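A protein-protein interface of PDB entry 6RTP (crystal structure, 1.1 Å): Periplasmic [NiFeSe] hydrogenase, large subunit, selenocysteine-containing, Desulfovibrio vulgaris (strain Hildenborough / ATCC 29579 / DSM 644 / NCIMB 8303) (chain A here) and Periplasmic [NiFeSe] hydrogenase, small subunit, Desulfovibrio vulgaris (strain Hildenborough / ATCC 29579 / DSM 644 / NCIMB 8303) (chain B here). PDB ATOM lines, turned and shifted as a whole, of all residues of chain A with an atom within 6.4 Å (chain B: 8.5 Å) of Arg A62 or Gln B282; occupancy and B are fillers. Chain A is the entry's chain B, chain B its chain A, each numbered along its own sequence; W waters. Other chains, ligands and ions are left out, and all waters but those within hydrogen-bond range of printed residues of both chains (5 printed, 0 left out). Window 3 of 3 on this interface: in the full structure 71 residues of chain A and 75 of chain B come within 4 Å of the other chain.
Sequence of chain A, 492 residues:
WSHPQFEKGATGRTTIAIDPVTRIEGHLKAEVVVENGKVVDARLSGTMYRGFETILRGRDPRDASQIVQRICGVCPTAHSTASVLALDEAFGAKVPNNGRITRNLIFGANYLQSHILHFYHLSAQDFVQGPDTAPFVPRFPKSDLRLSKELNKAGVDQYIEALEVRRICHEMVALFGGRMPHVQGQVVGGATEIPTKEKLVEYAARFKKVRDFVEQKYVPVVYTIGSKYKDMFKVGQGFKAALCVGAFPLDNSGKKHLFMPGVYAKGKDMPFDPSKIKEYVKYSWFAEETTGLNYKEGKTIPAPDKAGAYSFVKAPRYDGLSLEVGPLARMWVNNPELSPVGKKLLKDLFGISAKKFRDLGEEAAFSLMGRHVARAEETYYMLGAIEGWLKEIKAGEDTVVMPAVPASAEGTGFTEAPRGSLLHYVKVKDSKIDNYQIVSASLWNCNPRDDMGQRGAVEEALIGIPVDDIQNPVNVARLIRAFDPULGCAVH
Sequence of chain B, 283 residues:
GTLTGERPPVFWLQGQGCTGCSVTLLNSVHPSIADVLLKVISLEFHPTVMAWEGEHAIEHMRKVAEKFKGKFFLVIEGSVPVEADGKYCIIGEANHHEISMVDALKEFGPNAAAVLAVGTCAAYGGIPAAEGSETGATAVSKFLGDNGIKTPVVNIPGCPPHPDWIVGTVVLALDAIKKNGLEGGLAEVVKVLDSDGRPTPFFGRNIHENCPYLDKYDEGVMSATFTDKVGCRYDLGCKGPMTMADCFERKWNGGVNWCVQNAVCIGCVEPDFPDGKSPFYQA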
ATOM      1  N   ARG A  59      31.841   8.917 -13.316  1.00  0.00           N
ATOM      2  CA  ARG A  59      31.237   8.400 -12.102  1.00  0.00           C
ATOM      3  C   ARG A  59      32.303   8.004 -11.082  1.00  0.00           C
ATOM      4  O   ARG A  59      33.465   7.748 -11.413  1.00  0.00           O
ATOM      5  CB  ARG A  59      30.352   7.188 -12.419  1.00  0.00           C
ATOM      6  CG  ARG A  59      29.173   7.527 -13.297  1.00  0.00           C
ATOM      7  CD  ARG A  59      28.325   6.296 -13.717  1.00  0.00           C
ATOM      8  NE  ARG A  59      27.393   6.760 -14.730  1.00  0.00           N
ATOM      9  CZ  ARG A  59      26.216   7.321 -14.462  1.00  0.00           C
ATOM     10  NH1 ARG A  59      25.710   7.347 -13.238  1.00  0.00           N
ATOM     11  NH2 ARG A  59      25.524   7.839 -15.448  1.00  0.00           N
ATOM     12  N   ASP A  60      31.876   7.930  -9.829  1.00  0.00           N
ATOM     13  CA  ASP A  60      32.654   7.276  -8.792  1.00  0.00           C
ATOM     14  C   ASP A  60      32.974   5.867  -9.278  1.00  0.00           C
ATOM     15  O   ASP A  60      32.054   5.143  -9.691  1.00  0.00           O
ATOM     16  CB  ASP A  60      31.761   7.210  -7.549  1.00  0.00           C
ATOM     17  CG  ASP A  60      32.416   6.595  -6.323  1.00  0.00           C
ATOM     18  OD1 ASP A  60      33.245   5.665  -6.424  1.00  0.00           O
ATOM     19  OD2 ASP A  60      31.976   6.991  -5.221  1.00  0.00           O
ATOM     20  N   PRO A  61      34.248   5.452  -9.293  1.00  0.00           N
ATOM     21  CA  PRO A  61      34.551   4.129  -9.870  1.00  0.00           C
ATOM     22  C   PRO A  61      33.811   2.988  -9.197  1.00  0.00           C
ATOM     23  O   PRO A  61      33.499   1.984  -9.853  1.00  0.00           O
ATOM     24  CB  PRO A  61      36.069   4.020  -9.709  1.00  0.00           C
ATOM     25  CG  PRO A  61      36.536   5.441  -9.671  1.00  0.00           C
ATOM     26  CD  PRO A  61      35.473   6.186  -8.930  1.00  0.00           C
ATOM     27  N   ARG A  62      33.516   3.114  -7.902  1.00  0.00           N
ATOM     28  CA  ARG A  62      32.805   2.051  -7.205  1.00  0.00           C
ATOM     29  C   ARG A  62      31.413   1.827  -7.766  1.00  0.00           C
ATOM     30  O   ARG A  62      30.869   0.728  -7.622  1.00  0.00           O
ATOM     31  CB  ARG A  62      32.703   2.378  -5.723  1.00  0.00           C
ATOM     32  CG  ARG A  62      34.055   2.473  -5.036  1.00  0.00           C
ATOM     33  CD  ARG A  62      33.940   3.039  -3.633  1.00  0.00           C
ATOM     34  NE  ARG A  62      33.489   4.428  -3.642  1.00  0.00           N
ATOM     35  CZ  ARG A  62      33.298   5.150  -2.548  1.00  0.00           C
ATOM     36  NH1 ARG A  62      33.522   4.621  -1.352  1.00  0.00           N
ATOM     37  NH2 ARG A  62      32.881   6.402  -2.662  1.00  0.00           N
ATOM     38  N   ASP A  63      30.824   2.830  -8.408  1.00  0.00           N
ATOM     39  CA  ASP A  63      29.509   2.632  -9.002  1.00  0.00           C
ATOM     40  C   ASP A  63      29.545   1.613 -10.131  1.00  0.00           C
ATOM     41  O   ASP A  63      28.512   1.005 -10.432  1.00  0.00           O
ATOM     42  CB  ASP A  63      28.970   3.938  -9.584  1.00  0.00           C
ATOM     43  CG  ASP A  63      28.553   4.943  -8.541  1.00  0.00           C
ATOM     44  OD1 ASP A  63      28.617   4.656  -7.325  1.00  0.00           O
ATOM     45  OD2 ASP A  63      28.127   6.036  -8.989  1.00  0.00           O
ATOM     46  N   ALA A  64      30.710   1.397 -10.742  1.00  0.00           N
ATOM     47  CA  ALA A  64      30.777   0.525 -11.903  1.00  0.00           C
ATOM     48  C   ALA A  64      30.284  -0.875 -11.579  1.00  0.00           C
ATOM     49  O   ALA A  64      29.665  -1.526 -12.426  1.00  0.00           O
ATOM     50  CB  ALA A  64      32.203   0.451 -12.449  1.00  0.00           C
ATOM     51  N   SER A  65      30.560  -1.374 -10.374  1.00  0.00           N
ATOM     52  CA  SER A  65      30.219  -2.768 -10.082  1.00  0.00           C
ATOM     53  C   SER A  65      28.720  -2.984  -9.913  1.00  0.00           C
ATOM     54  O   SER A  65      28.275  -4.136  -9.899  1.00  0.00           O
ATOM     55  CB  SER A  65      31.034  -3.304  -8.906  1.00  0.00           C
ATOM     56  OG  SER A  65      30.944  -2.475  -7.777  1.00  0.00           O
ATOM     57  N   GLN A  66      27.936  -1.912  -9.840  1.00  0.00           N
ATOM     58  CA  GLN A  66      26.492  -1.997 -10.031  1.00  0.00           C
ATOM     59  C   GLN A  66      26.081  -1.692 -11.472  1.00  0.00           C
ATOM     60  O   GLN A  66      25.322  -2.456 -12.073  1.00  0.00           O
ATOM     61  CB  GLN A  66      25.772  -1.057  -9.059  1.00  0.00           C
ATOM     62  CG  GLN A  66      25.828  -1.566  -7.647  1.00  0.00           C
ATOM     63  CD  GLN A  66      25.175  -2.916  -7.529  1.00  0.00           C
ATOM     64  OE1 GLN A  66      24.028  -3.096  -7.939  1.00  0.00           O
ATOM     65  NE2 GLN A  66      25.914  -3.891  -7.008  1.00  0.00           N
ATOM     66  N   ILE A  67      26.560  -0.590 -12.045  1.00  0.00           N
ATOM     67  CA  ILE A  67      26.121  -0.189 -13.385  1.00  0.00           C
ATOM     68  C   ILE A  67      26.368  -1.299 -14.406  1.00  0.00           C
ATOM     69  O   ILE A  67      25.506  -1.577 -15.243  1.00  0.00           O
ATOM     70  CB  ILE A  67      26.786   1.133 -13.817  1.00  0.00           C
ATOM     71  CG1 ILE A  67      26.365   2.302 -12.920  1.00  0.00           C
ATOM     72  CG2 ILE A  67      26.493   1.444 -15.282  1.00  0.00           C
ATOM     73  CD1 ILE A  67      24.905   2.647 -12.945  1.00  0.00           C
ATOM     74  N   SER A  83      34.302  -6.431 -13.013  1.00  0.00           N
ATOM     75  CA  SER A  83      34.379  -5.056 -12.552  1.00  0.00           C
ATOM     76  C   SER A  83      35.075  -4.970 -11.202  1.00  0.00           C
ATOM     77  O   SER A  83      35.986  -4.157 -11.019  1.00  0.00           O
ATOM     78  CB  SER A  83      32.972  -4.484 -12.473  1.00  0.00           C
ATOM     79  OG  SER A  83      33.003  -3.132 -12.061  1.00  0.00           O
ATOM     80  N   LEU A  87      38.484  -3.046 -10.320  1.00  0.00           N
ATOM     81  CA  LEU A  87      38.540  -2.067  -9.243  1.00  0.00           C
ATOM     82  C   LEU A  87      39.513  -2.497  -8.152  1.00  0.00           C
ATOM     83  O   LEU A  87      40.264  -1.666  -7.629  1.00  0.00           O
ATOM     84  CB  LEU A  87      37.150  -1.863  -8.653  1.00  0.00           C
ATOM     85  CG  LEU A  87      36.111  -1.219  -9.575  1.00  0.00           C
ATOM     86  CD1 LEU A  87      34.741  -1.296  -8.953  1.00  0.00           C
ATOM     87  CD2 LEU A  87      36.471   0.229  -9.894  1.00  0.00           C
ATOM     88  N   PHE A  91      42.444  -0.023  -7.225  1.00  0.00           N
ATOM     89  CA  PHE A  91      42.444   0.548  -5.886  1.00  0.00           C
ATOM     90  C   PHE A  91      43.558  -0.022  -5.016  1.00  0.00           C
ATOM     91  O   PHE A  91      43.818   0.518  -3.934  1.00  0.00           O
ATOM     92  CB  PHE A  91      41.116   0.243  -5.170  1.00  0.00           C
ATOM     93  CG  PHE A  91      39.943   1.112  -5.576  1.00  0.00           C
ATOM     94  CD1 PHE A  91      39.674   1.432  -6.889  1.00  0.00           C
ATOM     95  CD2 PHE A  91      39.069   1.560  -4.604  1.00  0.00           C
ATOM     96  CE1 PHE A  91      38.581   2.208  -7.228  1.00  0.00           C
ATOM     97  CE2 PHE A  91      37.969   2.346  -4.946  1.00  0.00           C
ATOM     98  CZ  PHE A  91      37.733   2.653  -6.260  1.00  0.00           C
ATOM     99  N   VAL A 188      34.357  -3.687  -4.734  1.00  0.00           N
ATOM    100  CA  VAL A 188      35.802  -3.557  -4.573  1.00  0.00           C
ATOM    101  C   VAL A 188      36.157  -3.952  -3.145  1.00  0.00           C
ATOM    102  O   VAL A 188      35.493  -3.528  -2.197  1.00  0.00           O
ATOM    103  CB  VAL A 188      36.275  -2.136  -4.937  1.00  0.00           C
ATOM    104  CG1 VAL A 188      35.750  -1.079  -3.977  1.00  0.00           C
ATOM    105  CG2 VAL A 188      37.801  -2.094  -5.012  1.00  0.00           C
ATOM    106  N   MET A 402      37.875  -2.147   3.042  1.00  0.00           N
ATOM    107  CA  MET A 402      37.229  -0.878   2.691  1.00  0.00           C
ATOM    108  C   MET A 402      38.292   0.099   2.183  1.00  0.00           C
ATOM    109  O   MET A 402      38.790   0.948   2.938  1.00  0.00           O
ATOM    110  CB  MET A 402      36.459  -0.300   3.885  1.00  0.00           C
ATOM    111  CG  MET A 402      35.380  -1.216   4.445  1.00  0.00           C
ATOM    112  SD  MET A 402      34.023  -1.557   3.296  1.00  0.00           S
ATOM    113  CE  MET A 402      33.357   0.091   3.073  1.00  0.00           C
ATOM    114  N   PRO A 403      38.663   0.019   0.902  1.00  0.00           N
ATOM    115  CA  PRO A 403      39.762   0.852   0.394  1.00  0.00           C
ATOM    116  C   PRO A 403      39.313   2.238  -0.042  1.00  0.00           C
ATOM    117  O   PRO A 403      38.241   2.422  -0.623  1.00  0.00           O
ATOM    118  CB  PRO A 403      40.229   0.069  -0.836  1.00  0.00           C
ATOM    119  CG  PRO A 403      38.964  -0.523  -1.346  1.00  0.00           C
ATOM    120  CD  PRO A 403      38.185  -0.924  -0.129  1.00  0.00           C
ATOM    121  N   VAL A 405      39.153   5.509  -2.380  1.00  0.00           N
ATOM    122  CA  VAL A 405      39.144   5.691  -3.841  1.00  0.00           C
ATOM    123  C   VAL A 405      40.422   6.407  -4.258  1.00  0.00           C
ATOM    124  O   VAL A 405      40.721   7.488  -3.720  1.00  0.00           O
ATOM    125  CB  VAL A 405      37.916   6.503  -4.272  1.00  0.00           C
ATOM    126  CG1 VAL A 405      37.974   6.793  -5.779  1.00  0.00           C
ATOM    127  CG2 VAL A 405      36.616   5.784  -3.913  1.00  0.00           C
ATOM    128  N   LYS A 432      37.539   9.774 -10.604  1.00  0.00           N
ATOM    129  CA  LYS A 432      36.363   9.410 -11.383  1.00  0.00           C
ATOM    130  C   LYS A 432      36.772   8.528 -12.553  1.00  0.00           C
ATOM    131  O   LYS A 432      37.941   8.450 -12.929  1.00  0.00           O
ATOM    132  CB  LYS A 432      35.649  10.655 -11.919  1.00  0.00           C
ATOM    133  CG  LYS A 432      35.196  11.638 -10.843  1.00  0.00           C
ATOM    134  CD  LYS A 432      34.228  11.016  -9.843  1.00  0.00           C
ATOM    135  CE  LYS A 432      33.894  11.969  -8.689  1.00  0.00           C
ATOM    136  NZ  LYS A 432      33.026  11.322  -7.661  1.00  0.00           N
ATOM    137  N   ILE A 433      35.791   7.842 -13.129  1.00  0.00           N
ATOM    138  CA  ILE A 433      36.067   7.008 -14.292  1.00  0.00           C
ATOM    139  C   ILE A 433      36.423   7.896 -15.479  1.00  0.00           C
ATOM    140  O   ILE A 433      35.602   8.699 -15.940  1.00  0.00           O
ATOM    141  CB  ILE A 433      34.871   6.104 -14.624  1.00  0.00           C
ATOM    142  CG1 ILE A 433      34.625   5.125 -13.482  1.00  0.00           C
ATOM    143  CG2 ILE A 433      35.122   5.360 -15.944  1.00  0.00           C
ATOM    144  CD1 ILE A 433      33.377   4.262 -13.691  1.00  0.00           C
ATOM    145  N   PHE B 226      30.987  -3.007   5.148  1.00  0.00           N
ATOM    146  CA  PHE B 226      29.781  -3.678   4.695  1.00  0.00           C
ATOM    147  C   PHE B 226      29.463  -4.895   5.550  1.00  0.00           C
ATOM    148  O   PHE B 226      28.289  -5.234   5.737  1.00  0.00           O
ATOM    149  CB  PHE B 226      29.925  -4.143   3.245  1.00  0.00           C
ATOM    150  CG  PHE B 226      29.972  -3.030   2.230  1.00  0.00           C
ATOM    151  CD1 PHE B 226      28.827  -2.319   1.911  1.00  0.00           C
ATOM    152  CD2 PHE B 226      31.138  -2.735   1.547  1.00  0.00           C
ATOM    153  CE1 PHE B 226      28.864  -1.310   0.964  1.00  0.00           C
ATOM    154  CE2 PHE B 226      31.180  -1.729   0.613  1.00  0.00           C
ATOM    155  CZ  PHE B 226      30.038  -1.029   0.309  1.00  0.00           C
ATOM    156  N   ARG B 233      23.169   1.163   7.426  1.00  0.00           N
ATOM    157  CA  ARG B 233      23.962   1.202   6.206  1.00  0.00           C
ATOM    158  C   ARG B 233      24.002   2.583   5.540  1.00  0.00           C
ATOM    159  O   ARG B 233      24.541   2.713   4.429  1.00  0.00           O
ATOM    160  CB  ARG B 233      23.398   0.174   5.222  1.00  0.00           C
ATOM    161  CG  ARG B 233      23.659  -1.293   5.571  1.00  0.00           C
ATOM    162  CD  ARG B 233      22.917  -1.817   6.791  1.00  0.00           C
ATOM    163  NE  ARG B 233      22.797  -3.269   6.686  1.00  0.00           N
ATOM    164  CZ  ARG B 233      22.749  -4.134   7.694  1.00  0.00           C
ATOM    165  NH1 ARG B 233      22.815  -3.744   8.957  1.00  0.00           N
ATOM    166  NH2 ARG B 233      22.642  -5.422   7.418  1.00  0.00           N
ATOM    167  N   TYR B 234      23.470   3.611   6.196  1.00  0.00           N
ATOM    168  CA  TYR B 234      23.378   4.937   5.589  1.00  0.00           C
ATOM    169  C   TYR B 234      24.739   5.480   5.144  1.00  0.00           C
ATOM    170  O   TYR B 234      24.878   5.992   4.026  1.00  0.00           O
ATOM    171  CB  TYR B 234      22.713   5.895   6.570  1.00  0.00           C
ATOM    172  CG  TYR B 234      22.522   7.284   6.029  1.00  0.00           C
ATOM    173  CD1 TYR B 234      21.472   7.574   5.187  1.00  0.00           C
ATOM    174  CD2 TYR B 234      23.393   8.306   6.359  1.00  0.00           C
ATOM    175  CE1 TYR B 234      21.285   8.827   4.693  1.00  0.00           C
ATOM    176  CE2 TYR B 234      23.214   9.582   5.872  1.00  0.00           C
ATOM    177  CZ  TYR B 234      22.160   9.832   5.034  1.00  0.00           C
ATOM    178  OH  TYR B 234      21.975  11.099   4.539  1.00  0.00           O
ATOM    179  N   ASP B 235      25.758   5.413   6.011  1.00  0.00           N
ATOM    180  CA  ASP B 235      27.056   5.960   5.624  1.00  0.00           C
ATOM    181  C   ASP B 235      27.704   5.175   4.495  1.00  0.00           C
ATOM    182  O   ASP B 235      28.536   5.733   3.770  1.00  0.00           O
ATOM    183  CB  ASP B 235      28.027   5.983   6.807  1.00  0.00           C
ATOM    184  CG  ASP B 235      27.720   7.063   7.820  1.00  0.00           C
ATOM    185  OD1 ASP B 235      26.843   7.913   7.567  1.00  0.00           O
ATOM    186  OD2 ASP B 235      28.381   7.057   8.886  1.00  0.00           O
ATOM    187  N   LEU B 236      27.350   3.898   4.339  1.00  0.00           N
ATOM    188  CA  LEU B 236      27.826   3.068   3.245  1.00  0.00           C
ATOM    189  C   LEU B 236      27.082   3.338   1.945  1.00  0.00           C
ATOM    190  O   LEU B 236      27.427   2.740   0.924  1.00  0.00           O
ATOM    191  CB  LEU B 236      27.694   1.591   3.615  1.00  0.00           C
ATOM    192  CG  LEU B 236      28.574   1.118   4.773  1.00  0.00           C
ATOM    193  CD1 LEU B 236      28.098  -0.245   5.256  1.00  0.00           C
ATOM    194  CD2 LEU B 236      30.023   1.061   4.347  1.00  0.00           C
ATOM    195  N   GLY B 237      26.074   4.216   1.953  1.00  0.00           N
ATOM    196  CA  GLY B 237      25.385   4.651   0.756  1.00  0.00           C
ATOM    197  C   GLY B 237      23.918   4.263   0.642  1.00  0.00           C
ATOM    198  O   GLY B 237      23.303   4.540  -0.395  1.00  0.00           O
ATOM    199  N   CYS B 238      23.330   3.651   1.662  1.00  0.00           N
ATOM    200  CA  CYS B 238      21.959   3.162   1.539  1.00  0.00           C
ATOM    201  C   CYS B 238      21.002   4.285   1.150  1.00  0.00           C
ATOM    202  O   CYS B 238      20.954   5.332   1.807  1.00  0.00           O
ATOM    203  CB  CYS B 238      21.521   2.545   2.867  1.00  0.00           C
ATOM    204  SG  CYS B 238      19.896   1.748   2.756  1.00  0.00           S
ATOM    205  N   LYS B 239      20.194   4.038   0.114  1.00  0.00           N
ATOM    206  CA  LYS B 239      19.201   4.998  -0.353  1.00  0.00           C
ATOM    207  C   LYS B 239      17.787   4.645   0.086  1.00  0.00           C
ATOM    208  O   LYS B 239      16.815   5.178  -0.465  1.00  0.00           O
ATOM    209  CB  LYS B 239      19.258   5.131  -1.874  1.00  0.00           C
ATOM    210  CG  LYS B 239      20.643   5.532  -2.423  1.00  0.00           C
ATOM    211  CD  LYS B 239      21.246   6.742  -1.714  1.00  0.00           C
ATOM    212  CE  LYS B 239      22.509   7.283  -2.377  1.00  0.00           C
ATOM    213  NZ  LYS B 239      23.506   6.242  -2.566  1.00  0.00           N
ATOM    214  N   VAL B 264      23.659  -2.460   0.462  1.00  0.00           N
ATOM    215  CA  VAL B 264      22.887  -1.227   0.556  1.00  0.00           C
ATOM    216  C   VAL B 264      21.761  -1.290  -0.467  1.00  0.00           C
ATOM    217  O   VAL B 264      21.840  -2.020  -1.450  1.00  0.00           O
ATOM    218  CB  VAL B 264      23.767   0.020   0.277  1.00  0.00           C
ATOM    219  CG1 VAL B 264      24.900   0.133   1.292  1.00  0.00           C
ATOM    220  CG2 VAL B 264      24.340  -0.001  -1.129  1.00  0.00           C
ATOM    221  N   CYS B 265      20.704  -0.508  -0.226  1.00  0.00           N
ATOM    222  CA  CYS B 265      19.715  -0.210  -1.257  1.00  0.00           C
ATOM    223  C   CYS B 265      20.275   0.871  -2.168  1.00  0.00           C
ATOM    224  O   CYS B 265      20.859   1.850  -1.689  1.00  0.00           O
ATOM    225  CB  CYS B 265      18.411   0.254  -0.592  1.00  0.00           C
ATOM    226  SG  CYS B 265      17.096   0.829  -1.732  1.00  0.00           S
ATOM    227  N   LYS B 277      20.585   8.577  -7.551  1.00  0.00           N
ATOM    228  CA  LYS B 277      20.889   7.655  -6.467  1.00  0.00           C
ATOM    229  C   LYS B 277      22.382   7.396  -6.362  1.00  0.00           C
ATOM    230  O   LYS B 277      22.807   6.567  -5.549  1.00  0.00           O
ATOM    231  CB  LYS B 277      20.135   6.344  -6.695  1.00  0.00           C
ATOM    232  CG  LYS B 277      18.628   6.508  -6.603  1.00  0.00           C
ATOM    233  CD  LYS B 277      18.153   6.739  -5.175  1.00  0.00           C
ATOM    234  CE  LYS B 277      16.650   6.889  -5.097  1.00  0.00           C
ATOM    235  NZ  LYS B 277      16.203   8.236  -5.520  1.00  0.00           N
ATOM    236  N   SER B 278      23.187   8.103  -7.168  1.00  0.00           N
ATOM    237  CA  SER B 278      24.622   7.910  -7.271  1.00  0.00           C
ATOM    238  C   SER B 278      25.356   9.100  -6.674  1.00  0.00           C
ATOM    239  O   SER B 278      24.835  10.218  -6.704  1.00  0.00           O
ATOM    240  CB  SER B 278      25.044   7.800  -8.745  1.00  0.00           C
ATOM    241  OG  SER B 278      24.416   6.698  -9.368  1.00  0.00           O
ATOM    242  N   PRO B 279      26.572   8.912  -6.125  1.00  0.00           N
ATOM    243  CA  PRO B 279      27.292   7.641  -5.977  1.00  0.00           C
ATOM    244  C   PRO B 279      26.563   6.654  -5.073  1.00  0.00           C
ATOM    245  O   PRO B 279      25.910   7.059  -4.102  1.00  0.00           O
ATOM    246  CB  PRO B 279      28.624   8.072  -5.359  1.00  0.00           C
ATOM    247  CG  PRO B 279      28.827   9.471  -5.859  1.00  0.00           C
ATOM    248  CD  PRO B 279      27.449  10.064  -5.832  1.00  0.00           C
ATOM    249  N   PHE B 280      26.670   5.363  -5.402  1.00  0.00           N
ATOM    250  CA  PHE B 280      25.934   4.351  -4.656  1.00  0.00           C
ATOM    251  C   PHE B 280      26.527   4.095  -3.282  1.00  0.00           C
ATOM    252  O   PHE B 280      25.803   3.659  -2.380  1.00  0.00           O
ATOM    253  CB  PHE B 280      25.919   3.042  -5.448  1.00  0.00           C
ATOM    254  CG  PHE B 280      25.121   3.102  -6.716  1.00  0.00           C
ATOM    255  CD1 PHE B 280      23.824   3.584  -6.717  1.00  0.00           C
ATOM    256  CD2 PHE B 280      25.673   2.673  -7.911  1.00  0.00           C
ATOM    257  CE1 PHE B 280      23.091   3.620  -7.887  1.00  0.00           C
ATOM    258  CE2 PHE B 280      24.944   2.706  -9.082  1.00  0.00           C
ATOM    259  CZ  PHE B 280      23.644   3.195  -9.067  1.00  0.00           C
ATOM    260  N   TYR B 281      27.818   4.372  -3.089  1.00  0.00           N
ATOM    261  CA  TYR B 281      28.523   3.927  -1.895  1.00  0.00           C
ATOM    262  C   TYR B 281      28.944   5.071  -0.993  1.00  0.00           C
ATOM    263  O   TYR B 281      29.863   4.928  -0.180  1.00  0.00           O
ATOM    264  CB  TYR B 281      29.665   2.991  -2.264  1.00  0.00           C
ATOM    265  CG  TYR B 281      29.105   1.734  -2.897  1.00  0.00           C
ATOM    266  CD1 TYR B 281      28.321   0.849  -2.168  1.00  0.00           C
ATOM    267  CD2 TYR B 281      29.321   1.454  -4.237  1.00  0.00           C
ATOM    268  CE1 TYR B 281      27.794  -0.291  -2.753  1.00  0.00           C
ATOM    269  CE2 TYR B 281      28.809   0.311  -4.828  1.00  0.00           C
ATOM    270  CZ  TYR B 281      28.038  -0.552  -4.083  1.00  0.00           C
ATOM    271  OH  TYR B 281      27.533  -1.681  -4.696  1.00  0.00           O
ATOM    272  N   GLN B 282      28.255   6.192  -1.093  1.00  0.00           N
ATOM    273  CA  GLN B 282      28.320   7.194  -0.052  1.00  0.00           C
ATOM    274  C   GLN B 282      26.953   7.851   0.019  1.00  0.00           C
ATOM    275  O   GLN B 282      26.113   7.689  -0.874  1.00  0.00           O
ATOM    276  CB  GLN B 282      29.476   8.173  -0.271  1.00  0.00           C
ATOM    277  CG  GLN B 282      29.537   8.774  -1.635  1.00  0.00           C
ATOM    278  CD  GLN B 282      30.758   9.669  -1.822  1.00  0.00           C
ATOM    279  OE1 GLN B 282      31.890   9.289  -1.495  1.00  0.00           O
ATOM    280  NE2 GLN B 282      30.528  10.868  -2.331  1.00  0.00           N
ATOM    281  N   ALA B 283      26.713   8.536   1.123  1.00  0.00           N
ATOM    282  CA  ALA B 283      25.421   9.151   1.332  1.00  0.00           C
ATOM    283  C   ALA B 283      25.244  10.289   0.343  1.00  0.00           C
ATOM    284  O   ALA B 283      24.159  10.451  -0.213  1.00  0.00           O
ATOM    285  CB  ALA B 283      25.293   9.641   2.760  1.00  0.00           C
ATOM    286  OXT ALA B 283      26.182  11.039   0.065  1.00  0.00           O
HETATM  287  O   HOH W   1      29.981   4.878  -4.981  1.00  0.00           O
HETATM  288  O   HOH W   2      26.358   5.734 -11.025  1.00  0.00           O
HETATM  289  O   HOH W   3      28.852  -3.416  -6.299  1.00  0.00           O
HETATM  290  O   HOH W   4      32.074   9.714  -4.668  1.00  0.00           O
HETATM  291  O   HOH W   5      33.010   6.801   0.642  1.00  0.00           O
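The backbone NH of Phe B280 sits at hydrogen-bond distance from the side-chain carboxylate of Asp A63, 2.8 Å away. OE1 of Gln B282 sits at hydrogen-bond distance from NH2 of Arg A62, 3.3 Å away.
NZ of Lys B239 is in hydrogen-bond range of O of Pro B279. The side-chain amino group (NZ) of Lys B239 sits at hydrogen-bond distance from the backbone carbonyl oxygen (O) of Phe B280 (3.5 Å). NZ of Lys B239 is in hydrogen-bond range of O of Gln B282, 3.4 Å away. The side-chain carboxylate (OD2) of Asp A60 lies within salt-bridge range of the guanidinium group (NH2) of Arg A62. The backbone carbonyl oxygen of Arg A62 is in hydrogen-bond range of the side-chain hydroxyl of Ser A65.
Among the printed residues, merely in contact across the chains: Asp A60 with Pro B279 (3.5 Å), Arg A62 with Tyr B281 (3.5 Å), Asp A63 with Ser B278 (3.6 Å), Asp A63 with Pro B279 (3.5 Å), Gln A66 with Phe B280 (3.9 Å), Gln A66 with Tyr B281 (3.4 Å), Ile A67 with Phe B280 (3.9 Å), Met A402 with Phe B226 (3.6 Å) and Met A402 with Leu B236 (3.7 Å).
Arg A62 touches just these residues of chain B: Tyr B281 (3.5 Å) and Gln B282 (3.3 Å). Of chain A, only Arg A62 comes within 4 Å of Gln B282. No residue of chain B comes within 4 Å of Pro A61. Of the printed residues of chain B, Ile A67 touches Phe B280 (3.9 Å). Of the printed residues of chain A, Ser B278 touches Asp A63 (3.6 Å). The nearest residue of chain A that does not touch Gln B282 is Asp A60 (4.4 Å). The nearest printed residue of chain A that does not touch Leu B236 is Arg A62 (6.8 Å).
Hydrophobic or aromatic side chains of chain A within 4 Å of the printed part of chain B: Ile A67 and Met A402. Printed residues of chain B that touch a printed residue of chain A: Phe B226, Leu B236, Ser B278, Pro B279, Phe B280, Tyr B281 and Gln B282. Hydrophobic or aromatic side chains of chain B that line the printed part of chain A: Phe B226, Leu B236, Pro B279, Phe B280 and Tyr B281. Among the printed residues, 11 pairs touch across the chains. Among the printed residues, no Asp or Glu carboxylate lies within 4 Å of a Lys or Arg side-chain nitrogen of the other chain.
Water W3 lies within hydrogen-bond range of the side-chain hydroxyl (OH) of Tyr B281 (2.7 Å), the side-chain hydroxyl (OG) of Ser A65 (2.7 Å) and the side-chain amide nitrogen (NE2) of Gln A66 (3.1 Å). Water W4 lies within hydrogen-bond range of the side-chain carboxylate of Asp A60 (2.8 Å) and the side-chain amide nitrogen of Gln B282 (3.0 Å). Water W5 lies within hydrogen-bond range of NH1 of Arg A62 (3.0 Å) and OE1 of Gln B282 (3.5 Å).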
